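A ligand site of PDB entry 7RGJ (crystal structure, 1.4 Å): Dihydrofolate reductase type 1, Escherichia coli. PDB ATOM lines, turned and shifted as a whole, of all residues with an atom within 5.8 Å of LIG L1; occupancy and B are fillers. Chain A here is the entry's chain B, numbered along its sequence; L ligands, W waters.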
ATOM      1  N   MET A   6      14.151 -13.713 -13.216  1.00  0.00           N
ATOM      2  CA  MET A   6      13.507 -14.651 -14.132  1.00  0.00           C
ATOM      3  C   MET A   6      12.219 -15.180 -13.513  1.00  0.00           C
ATOM      4  O   MET A   6      12.216 -15.616 -12.356  1.00  0.00           O
ATOM      5  CB  MET A   6      14.440 -15.818 -14.483  1.00  0.00           C
ATOM      6  CG  MET A   6      13.901 -16.728 -15.542  1.00  0.00           C
ATOM      7  SD  MET A   6      15.211 -17.586 -16.403  1.00  0.00           S
ATOM      8  CE  MET A   6      14.454 -17.915 -17.992  1.00  0.00           C
ATOM      9  N   VAL A   7      11.127 -15.126 -14.276  1.00  0.00           N
ATOM     10  CA  VAL A   7       9.791 -15.492 -13.801  1.00  0.00           C
ATOM     11  C   VAL A   7       8.958 -15.974 -14.987  1.00  0.00           C
ATOM     12  O   VAL A   7       9.163 -15.566 -16.131  1.00  0.00           O
ATOM     13  CB  VAL A   7       9.113 -14.296 -13.095  1.00  0.00           C
ATOM     14  CG1 VAL A   7       8.849 -13.179 -14.110  1.00  0.00           C
ATOM     15  CG2 VAL A   7       7.822 -14.742 -12.377  1.00  0.00           C
ATOM     16  N   ALA A   8       7.999 -16.847 -14.703  1.00  0.00           N
ATOM     17  CA  ALA A   8       6.965 -17.243 -15.641  1.00  0.00           C
ATOM     18  C   ALA A   8       5.637 -16.744 -15.094  1.00  0.00           C
ATOM     19  O   ALA A   8       5.251 -17.094 -13.970  1.00  0.00           O
ATOM     20  CB  ALA A   8       6.935 -18.771 -15.785  1.00  0.00           C
ATOM     21  N   PRO A  19       2.230 -23.256  -2.494  1.00  0.00           N
ATOM     22  CA  PRO A  19       3.634 -23.592  -2.763  1.00  0.00           C
ATOM     23  C   PRO A  19       3.932 -24.021  -4.193  1.00  0.00           C
ATOM     24  O   PRO A  19       5.084 -24.338  -4.498  1.00  0.00           O
ATOM     25  CB  PRO A  19       3.867 -24.765  -1.791  1.00  0.00           C
ATOM     26  CG  PRO A  19       2.545 -25.451  -1.754  1.00  0.00           C
ATOM     27  CD  PRO A  19       1.500 -24.378  -1.871  1.00  0.00           C
ATOM     28  N   ILE A  21       3.569 -23.814  -8.616  1.00  0.00           N
ATOM     29  CA  ILE A  21       3.281 -23.094  -9.851  1.00  0.00           C
ATOM     30  C   ILE A  21       2.148 -23.846 -10.550  1.00  0.00           C
ATOM     31  O   ILE A  21       2.317 -25.030 -10.876  1.00  0.00           O
ATOM     32  CB  ILE A  21       4.529 -23.033 -10.744  1.00  0.00           C
ATOM     33  CG1 ILE A  21       5.617 -22.228 -10.036  1.00  0.00           C
ATOM     34  CG2 ILE A  21       4.184 -22.440 -12.108  1.00  0.00           C
ATOM     35  CD1 ILE A  21       6.968 -22.223 -10.755  1.00  0.00           C
ATOM     36  N   GLU A  28       9.078 -24.846 -21.325  1.00  0.00           N
ATOM     37  CA  GLU A  28       9.422 -23.551 -20.740  1.00  0.00           C
ATOM     38  C   GLU A  28      10.530 -23.686 -19.702  1.00  0.00           C
ATOM     39  O   GLU A  28      11.402 -22.814 -19.598  1.00  0.00           O
ATOM     40  CB  GLU A  28       8.183 -22.887 -20.135  1.00  0.00           C
ATOM     41  CG  GLU A  28       8.305 -21.374 -19.938  1.00  0.00           C
ATOM     42  CD  GLU A  28       9.151 -20.977 -18.734  1.00  0.00           C
ATOM     43  OE1 GLU A  28       9.006 -21.602 -17.656  1.00  0.00           O
ATOM     44  OE2 GLU A  28       9.940 -20.024 -18.850  1.00  0.00           O
ATOM     45  N   GLN A  29      10.525 -24.786 -18.951  1.00  0.00           N
ATOM     46  CA  GLN A  29      11.534 -25.010 -17.930  1.00  0.00           C
ATOM     47  C   GLN A  29      12.946 -25.053 -18.514  1.00  0.00           C
ATOM     48  O   GLN A  29      13.905 -24.823 -17.770  1.00  0.00           O
ATOM     49  CB  GLN A  29      11.201 -26.328 -17.219  1.00  0.00           C
ATOM     50  CG  GLN A  29      11.874 -26.578 -15.892  1.00  0.00           C
ATOM     51  CD  GLN A  29      11.308 -27.815 -15.212  1.00  0.00           C
ATOM     52  OE1 GLN A  29      10.549 -27.715 -14.248  1.00  0.00           O
ATOM     53  NE2 GLN A  29      11.644 -28.984 -15.733  1.00  0.00           N
ATOM     54  N   LEU A  31      14.165 -22.891 -20.577  1.00  0.00           N
ATOM     55  CA  LEU A  31      14.678 -21.522 -20.519  1.00  0.00           C
ATOM     56  C   LEU A  31      15.245 -21.247 -19.140  1.00  0.00           C
ATOM     57  O   LEU A  31      16.348 -20.690 -19.005  1.00  0.00           O
ATOM     58  CB  LEU A  31      13.553 -20.525 -20.844  1.00  0.00           C
ATOM     59  CG  LEU A  31      13.041 -20.556 -22.291  1.00  0.00           C
ATOM     60  CD1 LEU A  31      11.680 -19.883 -22.366  1.00  0.00           C
ATOM     61  CD2 LEU A  31      14.037 -19.878 -23.246  1.00  0.00           C
ATOM     62  N   PHE A  32      14.511 -21.649 -18.100  1.00  0.00           N
ATOM     63  CA  PHE A  32      14.975 -21.469 -16.725  1.00  0.00           C
ATOM     64  C   PHE A  32      16.267 -22.239 -16.478  1.00  0.00           C
ATOM     65  O   PHE A  32      17.224 -21.690 -15.933  1.00  0.00           O
ATOM     66  CB  PHE A  32      13.879 -21.925 -15.766  1.00  0.00           C
ATOM     67  CG  PHE A  32      14.254 -21.824 -14.309  1.00  0.00           C
ATOM     68  CD1 PHE A  32      14.297 -20.594 -13.671  1.00  0.00           C
ATOM     69  CD2 PHE A  32      14.568 -22.969 -13.593  1.00  0.00           C
ATOM     70  CE1 PHE A  32      14.651 -20.500 -12.322  1.00  0.00           C
ATOM     71  CE2 PHE A  32      14.925 -22.883 -12.239  1.00  0.00           C
ATOM     72  CZ  PHE A  32      14.962 -21.637 -11.612  1.00  0.00           C
ATOM     73  N   LYS A  33      16.321 -23.498 -16.920  1.00  0.00           N
ATOM     74  CA  LYS A  33      17.533 -24.295 -16.740  1.00  0.00           C
ATOM     75  C   LYS A  33      18.723 -23.660 -17.428  1.00  0.00           C
ATOM     76  O   LYS A  33      19.827 -23.595 -16.864  1.00  0.00           O
ATOM     77  CB  LYS A  33      17.338 -25.716 -17.276  1.00  0.00           C
ATOM     78  CG  LYS A  33      16.324 -26.522 -16.526  1.00  0.00           C
ATOM     79  CD  LYS A  33      16.903 -26.914 -15.203  1.00  0.00           C
ATOM     80  CE  LYS A  33      15.826 -26.923 -14.167  1.00  0.00           C
ATOM     81  NZ  LYS A  33      15.845 -25.818 -13.188  1.00  0.00           N
ATOM     82  N   VAL A  43      16.641 -16.370  -3.699  1.00  0.00           N
ATOM     83  CA  VAL A  43      15.289 -16.916  -3.540  1.00  0.00           C
ATOM     84  C   VAL A  43      14.779 -16.718  -2.121  1.00  0.00           C
ATOM     85  O   VAL A  43      15.529 -16.769  -1.135  1.00  0.00           O
ATOM     86  CB  VAL A  43      15.195 -18.402  -3.914  1.00  0.00           C
ATOM     87  CG1 VAL A  43      15.408 -18.610  -5.421  1.00  0.00           C
ATOM     88  CG2 VAL A  43      16.192 -19.229  -3.102  1.00  0.00           C
ATOM     89  N   THR A  47       9.942 -20.366  -1.645  1.00  0.00           N
ATOM     90  CA  THR A  47      10.287 -20.907  -2.951  1.00  0.00           C
ATOM     91  C   THR A  47      11.392 -21.948  -2.839  1.00  0.00           C
ATOM     92  O   THR A  47      11.349 -22.979  -3.504  1.00  0.00           O
ATOM     93  CB  THR A  47      10.692 -19.761  -3.870  1.00  0.00           C
ATOM     94  OG1 THR A  47       9.535 -18.970  -4.178  1.00  0.00           O
ATOM     95  CG2 THR A  47      11.265 -20.285  -5.202  1.00  0.00           C
ATOM     96  N   SER A  50      10.055 -25.257  -1.817  1.00  0.00           N
ATOM     97  CA  SER A  50       9.317 -25.933  -2.875  1.00  0.00           C
ATOM     98  C   SER A  50      10.237 -26.502  -3.950  1.00  0.00           C
ATOM     99  O   SER A  50      10.101 -27.655  -4.358  1.00  0.00           O
ATOM    100  CB  SER A  50       8.296 -24.983  -3.501  1.00  0.00           C
ATOM    101  OG  SER A  50       7.328 -24.589  -2.555  1.00  0.00           O
ATOM    102  N   MET A  51      11.191 -25.691  -4.427  1.00  0.00           N
ATOM    103  CA  MET A  51      12.046 -26.114  -5.533  1.00  0.00           C
ATOM    104  C   MET A  51      13.131 -27.081  -5.091  1.00  0.00           C
ATOM    105  O   MET A  51      13.465 -28.021  -5.813  1.00  0.00           O
ATOM    106  CB  MET A  51      12.637 -24.880  -6.232  1.00  0.00           C
ATOM    107  CG  MET A  51      13.805 -25.158  -7.159  1.00  0.00           C
ATOM    108  SD  MET A  51      14.677 -23.636  -7.640  1.00  0.00           S
ATOM    109  CE  MET A  51      14.511 -22.664  -6.151  1.00  0.00           C
ATOM    110  N   LEU A  54      18.385 -27.677  -6.657  1.00  0.00           N
ATOM    111  CA  LEU A  54      18.599 -28.413  -7.895  1.00  0.00           C
ATOM    112  C   LEU A  54      20.054 -28.332  -8.347  1.00  0.00           C
ATOM    113  O   LEU A  54      20.743 -27.346  -8.073  1.00  0.00           O
ATOM    114  CB  LEU A  54      17.652 -27.925  -8.974  1.00  0.00           C
ATOM    115  CG  LEU A  54      16.191 -28.077  -8.512  1.00  0.00           C
ATOM    116  CD1 LEU A  54      15.210 -27.516  -9.526  1.00  0.00           C
ATOM    117  CD2 LEU A  54      15.877 -29.532  -8.200  1.00  0.00           C
ATOM    118  N   SER A  97      15.076 -15.188  -8.365  1.00  0.00           N
ATOM    119  CA  SER A  97      14.331 -16.350  -8.855  1.00  0.00           C
ATOM    120  C   SER A  97      13.087 -16.647  -8.025  1.00  0.00           C
ATOM    121  O   SER A  97      12.592 -17.777  -8.045  1.00  0.00           O
ATOM    122  CB  SER A  97      15.245 -17.567  -8.960  1.00  0.00           C
ATOM    123  OG  SER A  97      16.357 -17.241  -9.786  1.00  0.00           O
ATOM    124  N   GLY A  98      12.559 -15.652  -7.319  1.00  0.00           N
ATOM    125  CA  GLY A  98      11.244 -15.749  -6.695  1.00  0.00           C
ATOM    126  C   GLY A  98      11.349 -15.980  -5.199  1.00  0.00           C
ATOM    127  O   GLY A  98      12.437 -16.096  -4.629  1.00  0.00           O
ATOM    128  N   TYR A 103      10.315 -11.034  -5.519  1.00  0.00           N
ATOM    129  CA  TYR A 103      10.159 -10.236  -6.734  1.00  0.00           C
ATOM    130  C   TYR A 103       9.707  -8.814  -6.410  1.00  0.00           C
ATOM    131  O   TYR A 103      10.217  -7.845  -6.985  1.00  0.00           O
ATOM    132  CB  TYR A 103       9.143 -10.878  -7.666  1.00  0.00           C
ATOM    133  CG  TYR A 103       9.556 -12.173  -8.316  1.00  0.00           C
ATOM    134  CD1 TYR A 103      10.792 -12.307  -8.950  1.00  0.00           C
ATOM    135  CD2 TYR A 103       8.665 -13.231  -8.400  1.00  0.00           C
ATOM    136  CE1 TYR A 103      11.152 -13.500  -9.590  1.00  0.00           C
ATOM    137  CE2 TYR A 103       8.992 -14.414  -9.044  1.00  0.00           C
ATOM    138  CZ  TYR A 103      10.243 -14.548  -9.653  1.00  0.00           C
ATOM    139  OH  TYR A 103      10.538 -15.724 -10.270  1.00  0.00           O
ATOM    140  N   HIS A 114      13.803 -11.565 -17.432  1.00  0.00           N
ATOM    141  CA  HIS A 114      13.480 -12.713 -18.274  1.00  0.00           C
ATOM    142  C   HIS A 114      12.059 -13.095 -17.902  1.00  0.00           C
ATOM    143  O   HIS A 114      11.829 -13.636 -16.805  1.00  0.00           O
ATOM    144  CB  HIS A 114      14.401 -13.877 -17.965  1.00  0.00           C
ATOM    145  CG  HIS A 114      15.825 -13.627 -18.308  1.00  0.00           C
ATOM    146  ND1 HIS A 114      16.388 -14.037 -19.492  1.00  0.00           N
ATOM    147  CD2 HIS A 114      16.814 -13.002 -17.620  1.00  0.00           C
ATOM    148  CE1 HIS A 114      17.659 -13.681 -19.531  1.00  0.00           C
ATOM    149  NE2 HIS A 114      17.942 -13.051 -18.403  1.00  0.00           N
ATOM    150  N   ILE A 115      11.100 -12.800 -18.777  1.00  0.00           N
ATOM    151  CA  ILE A 115       9.682 -13.027 -18.478  1.00  0.00           C
ATOM    152  C   ILE A 115       9.116 -13.992 -19.510  1.00  0.00           C
ATOM    153  O   ILE A 115       9.132 -13.702 -20.717  1.00  0.00           O
ATOM    154  CB  ILE A 115       8.880 -11.727 -18.479  1.00  0.00           C
ATOM    155  CG1 ILE A 115       9.423 -10.779 -17.405  1.00  0.00           C
ATOM    156  CG2 ILE A 115       7.405 -12.056 -18.238  1.00  0.00           C
ATOM    157  CD1 ILE A 115       8.660  -9.468 -17.285  1.00  0.00           C
ATOM    158  N   SER A 116       8.598 -15.116 -19.039  1.00  0.00           N
ATOM    159  CA  SER A 116       7.853 -16.039 -19.881  1.00  0.00           C
ATOM    160  C   SER A 116       6.374 -15.846 -19.573  1.00  0.00           C
ATOM    161  O   SER A 116       5.950 -16.046 -18.434  1.00  0.00           O
ATOM    162  CB  SER A 116       8.278 -17.469 -19.606  1.00  0.00           C
ATOM    163  OG  SER A 116       9.663 -17.630 -19.962  1.00  0.00           O
HETATM  164  C1  LIG L   1      10.194 -21.150 -14.249  1.00  0.00           C
HETATM  165  C2  LIG L   1      10.678 -20.520 -13.121  1.00  0.00           C
HETATM  166  C3  LIG L   1      11.185 -19.222 -13.214  1.00  0.00           C
HETATM  167  N1  LIG L   1      11.185 -18.590 -14.385  1.00  0.00           N
HETATM  168  N2  LIG L   1      10.212 -20.478 -15.409  1.00  0.00           N
HETATM  169  C4  LIG L   1      10.720 -19.233 -15.452  1.00  0.00           C
HETATM  170  C5  LIG L   1      10.673 -21.174 -11.852  1.00  0.00           C
HETATM  171  C6  LIG L   1      10.696 -21.664 -10.747  1.00  0.00           C
HETATM  172  C7  LIG L   1      10.764 -22.147  -9.367  1.00  0.00           C
HETATM  173  C8  LIG L   1      12.032 -21.624  -8.683  1.00  0.00           C
HETATM  174  C9  LIG L   1      10.641 -23.524  -9.230  1.00  0.00           C
HETATM  175  C10 LIG L   1      11.305 -24.436 -10.036  1.00  0.00           C
HETATM  176  C11 LIG L   1      11.107 -25.802  -9.789  1.00  0.00           C
HETATM  177  C12 LIG L   1      11.759 -26.720 -10.615  1.00  0.00           C
HETATM  178  C13 LIG L   1      11.784 -28.083 -10.338  1.00  0.00           C
HETATM  179  C14 LIG L   1      12.430 -28.985 -11.175  1.00  0.00           C
HETATM  180  C15 LIG L   1      13.074 -28.512 -12.302  1.00  0.00           C
HETATM  181  C16 LIG L   1      13.723 -29.410 -13.152  1.00  0.00           C
HETATM  182  C17 LIG L   1      13.049 -27.150 -12.578  1.00  0.00           C
HETATM  183  C18 LIG L   1      12.409 -26.250 -11.749  1.00  0.00           C
HETATM  184  C19 LIG L   1      10.264 -26.207  -8.822  1.00  0.00           C
HETATM  185  C20 LIG L   1       8.748 -27.295  -7.620  1.00  0.00           C
HETATM  186  C21 LIG L   1       9.628 -25.319  -8.064  1.00  0.00           C
HETATM  187  C22 LIG L   1       9.812 -24.014  -8.245  1.00  0.00           C
HETATM  188  C23 LIG L   1       9.619 -22.432 -14.205  1.00  0.00           C
HETATM  189  C24 LIG L   1      10.542 -23.483 -14.786  1.00  0.00           C
HETATM  190  N3  LIG L   1      10.740 -18.593 -16.623  1.00  0.00           N
HETATM  191  N4  LIG L   1      11.645 -18.605 -12.127  1.00  0.00           N
HETATM  192  N5  LIG L   1      13.717 -30.779 -12.615  1.00  0.00           N
HETATM  193  O1  LIG L   1       9.916 -27.474  -8.426  1.00  0.00           O
HETATM  194  O2  LIG L   1       8.841 -25.943  -7.126  1.00  0.00           O
HETATM  195  P1  LG2 L   2       8.851 -16.310  -1.234  1.00  0.00           P
HETATM  196  O1  LG2 L   2       9.094 -14.959  -1.815  1.00  0.00           O
HETATM  197  O2  LG2 L   2       9.388 -17.503  -1.987  1.00  0.00           O
HETATM  198  O3  LG2 L   2       9.469 -16.417   0.287  1.00  0.00           O
HETATM  199  C1  LG2 L   2       8.918 -15.564   1.274  1.00  0.00           C
HETATM  200  C2  LG2 L   2       9.734 -15.812   2.581  1.00  0.00           C
HETATM  201  O4  LG2 L   2      11.194 -15.258   2.250  1.00  0.00           O
HETATM  202  C3  LG2 L   2       9.358 -15.101   3.564  1.00  0.00           C
HETATM  203  O5  LG2 L   2       8.341 -15.787   4.358  1.00  0.00           O
HETATM  204  C4  LG2 L   2      10.764 -14.964   4.463  1.00  0.00           C
HETATM  205  O6  LG2 L   2      11.083 -16.257   4.987  1.00  0.00           O
HETATM  206  C5  LG2 L   2      11.670 -14.647   3.555  1.00  0.00           C
HETATM  207  N1  LG2 L   2      11.840 -13.207   3.282  1.00  0.00           N
HETATM  208  C6  LG2 L   2      11.130 -12.414   2.485  1.00  0.00           C
HETATM  209  N2  LG2 L   2      11.631 -11.187   2.510  1.00  0.00           N
HETATM  210  C7  LG2 L   2      12.703 -11.191   3.319  1.00  0.00           C
HETATM  211  C8  LG2 L   2      13.654 -10.239   3.763  1.00  0.00           C
HETATM  212  N3  LG2 L   2      13.592  -8.867   3.305  1.00  0.00           N
HETATM  213  N4  LG2 L   2      14.608 -10.643   4.598  1.00  0.00           N
HETATM  214  C9  LG2 L   2      14.679 -11.902   5.031  1.00  0.00           C
HETATM  215  N5  LG2 L   2      13.817 -12.824   4.633  1.00  0.00           N
HETATM  216  C10 LG2 L   2      12.836 -12.472   3.796  1.00  0.00           C
HETATM  217  O7  LG2 L   2       7.272 -16.592  -0.907  1.00  0.00           O
HETATM  218  P2  LG2 L   2       5.935 -16.251  -1.768  1.00  0.00           P
HETATM  219  O8  LG2 L   2       4.824 -16.880  -0.952  1.00  0.00           O
HETATM  220  O9  LG2 L   2       5.824 -14.776  -1.985  1.00  0.00           O
HETATM  221  O10 LG2 L   2       6.146 -16.991  -3.208  1.00  0.00           O
HETATM  222  C11 LG2 L   2       6.167 -18.403  -3.305  1.00  0.00           C
HETATM  223  C12 LG2 L   2       5.391 -18.746  -4.434  1.00  0.00           C
HETATM  224  O11 LG2 L   2       6.030 -18.133  -5.649  1.00  0.00           O
HETATM  225  C13 LG2 L   2       5.338 -20.299  -4.762  1.00  0.00           C
HETATM  226  O12 LG2 L   2       3.940 -20.636  -5.223  1.00  0.00           O
HETATM  227  C14 LG2 L   2       6.134 -20.447  -5.703  1.00  0.00           C
HETATM  228  O13 LG2 L   2       5.841 -21.635  -6.546  1.00  0.00           O
HETATM  229  C15 LG2 L   2       5.934 -19.035  -6.557  1.00  0.00           C
HETATM  230  N6  LG2 L   2       6.957 -18.887  -7.531  1.00  0.00           N
HETATM  231  C16 LG2 L   2       6.552 -18.762  -8.888  1.00  0.00           C
HETATM  232  C17 LG2 L   2       7.612 -18.644  -9.942  1.00  0.00           C
HETATM  233  C18 LG2 L   2       7.135 -18.494 -11.353  1.00  0.00           C
HETATM  234  O14 LG2 L   2       5.983 -18.636 -11.709  1.00  0.00           O
HETATM  235  N7  LG2 L   2       8.193 -18.174 -12.248  1.00  0.00           N
HETATM  236  C19 LG2 L   2       9.117 -18.636  -9.638  1.00  0.00           C
HETATM  237  C20 LG2 L   2       9.422 -18.838  -8.155  1.00  0.00           C
HETATM  238  C21 LG2 L   2       8.327 -18.913  -7.148  1.00  0.00           C
HETATM  239  P3  LG2 L   2      10.671 -16.800   6.504  1.00  0.00           P
HETATM  240  O15 LG2 L   2       9.168 -17.017   6.502  1.00  0.00           O
HETATM  241  O16 LG2 L   2      11.098 -15.724   7.459  1.00  0.00           O
HETATM  242  O17 LG2 L   2      11.391 -18.099   6.640  1.00  0.00           O
HETATM  243  O   HOH W   1      11.514 -16.259 -18.186  1.00  0.00           O
HETATM  244  O   HOH W   2       7.122 -24.041  -6.856  1.00  0.00           O
HETATM  245  O   HOH W   3       5.866 -25.688  -8.527  1.00  0.00           O
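Water W2 lies within hydrogen-bond range of an oxygen (O2) of LIG L1, an oxygen (O13) of LG2 L2 and the backbone carbonyl oxygen of Pro 19. Water W1 lies within hydrogen-bond range of OG of Ser 116 (2.9 Å), N3 of LIG L1 (2.9 Å), O of His 114 (3.0 Å) and O of Val 7 (3.2 Å). Water W3 lies within hydrogen-bond range of the backbone NH of Ile 21 and an oxygen (O2) of LIG L1.
The backbone carbonyl oxygen (O) of Ser 50 lies close to an oxygen (O2) of LIG L1, at 3.5 Å. N of Ala 8 touches N1 of LIG L1, 3.6 Å away. Ile 21 touches LIG L1 (CD1 to C6, 3.8 Å). Gln 29 touches LIG L1. Phe 32 touches LIG L1 (CD1 to C3, 3.4 Å). NZ of Lys 33 touches C17 of LIG L1 (3.2 Å). CG2 of Thr 47 touches C8 of LIG L1, at 3.8 Å. Met 51 touches LIG L1 (SD to C8, 3.5 Å). CD1 of Leu 54 touches C14 of LIG L1 (3.6 Å). Ser 97 touches LIG L1. OH of Tyr 103 touches N4 of LIG L1, at 3.6 Å. OG of Ser 116 touches N3 of LIG L1, at 3.6 Å. Hydrophobic or aromatic side chains that line LIG L1: Met 6, Ala 8, Ile 21, Phe 32, Met 51 and Leu 54. Along chain A the residues within 4 Å of LIG L1 span positions 6 to 116.
OG1 of Thr 47 lies within hydrogen-bond range of O2 of LG2 L2 (2.6 Å). The side-chain carboxylate of Glu 28 lies within hydrogen-bond range of a nitrogen (N3) of LIG L1, at 2.8 Å. The backbone carbonyl oxygen (O) of Pro 19 is in hydrogen-bond range of an oxygen (O13) of LG2 L2 (3.5 Å). O of Val 7 sits at hydrogen-bond distance from N3 of LIG L1 (3.4 Å). The backbone NH (N) of Thr 47 lies within hydrogen-bond range of an oxygen (O2) of LG2 L2. A nitrogen (N4) of LIG L1 lies within hydrogen-bond range of the backbone carbonyl oxygen (O) of Met 6 (3.1 Å). N of Val 7 lies close to N1 of LIG L1 (3.5 Å).
OG of Ser 50 is in hydrogen-bond range of O of Pro 19, at 3.0 Å. The backbone carbonyl oxygen of Met 6 is in hydrogen-bond range of the side-chain hydroxyl of Tyr 103 (2.7 Å). The backbone carbonyl oxygen (O) of Val 7 is in hydrogen-bond range of the backbone NH (N) of Ser 116 (3.0 Å). The backbone carbonyl oxygen (O) of His 114 is in hydrogen-bond range of the backbone NH (N) of Val 7, at 3.0 Å. The side-chain carboxylate (OE2) of Glu 28 is in hydrogen-bond range of the side-chain hydroxyl (OG) of Ser 116, 2.7 Å away.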
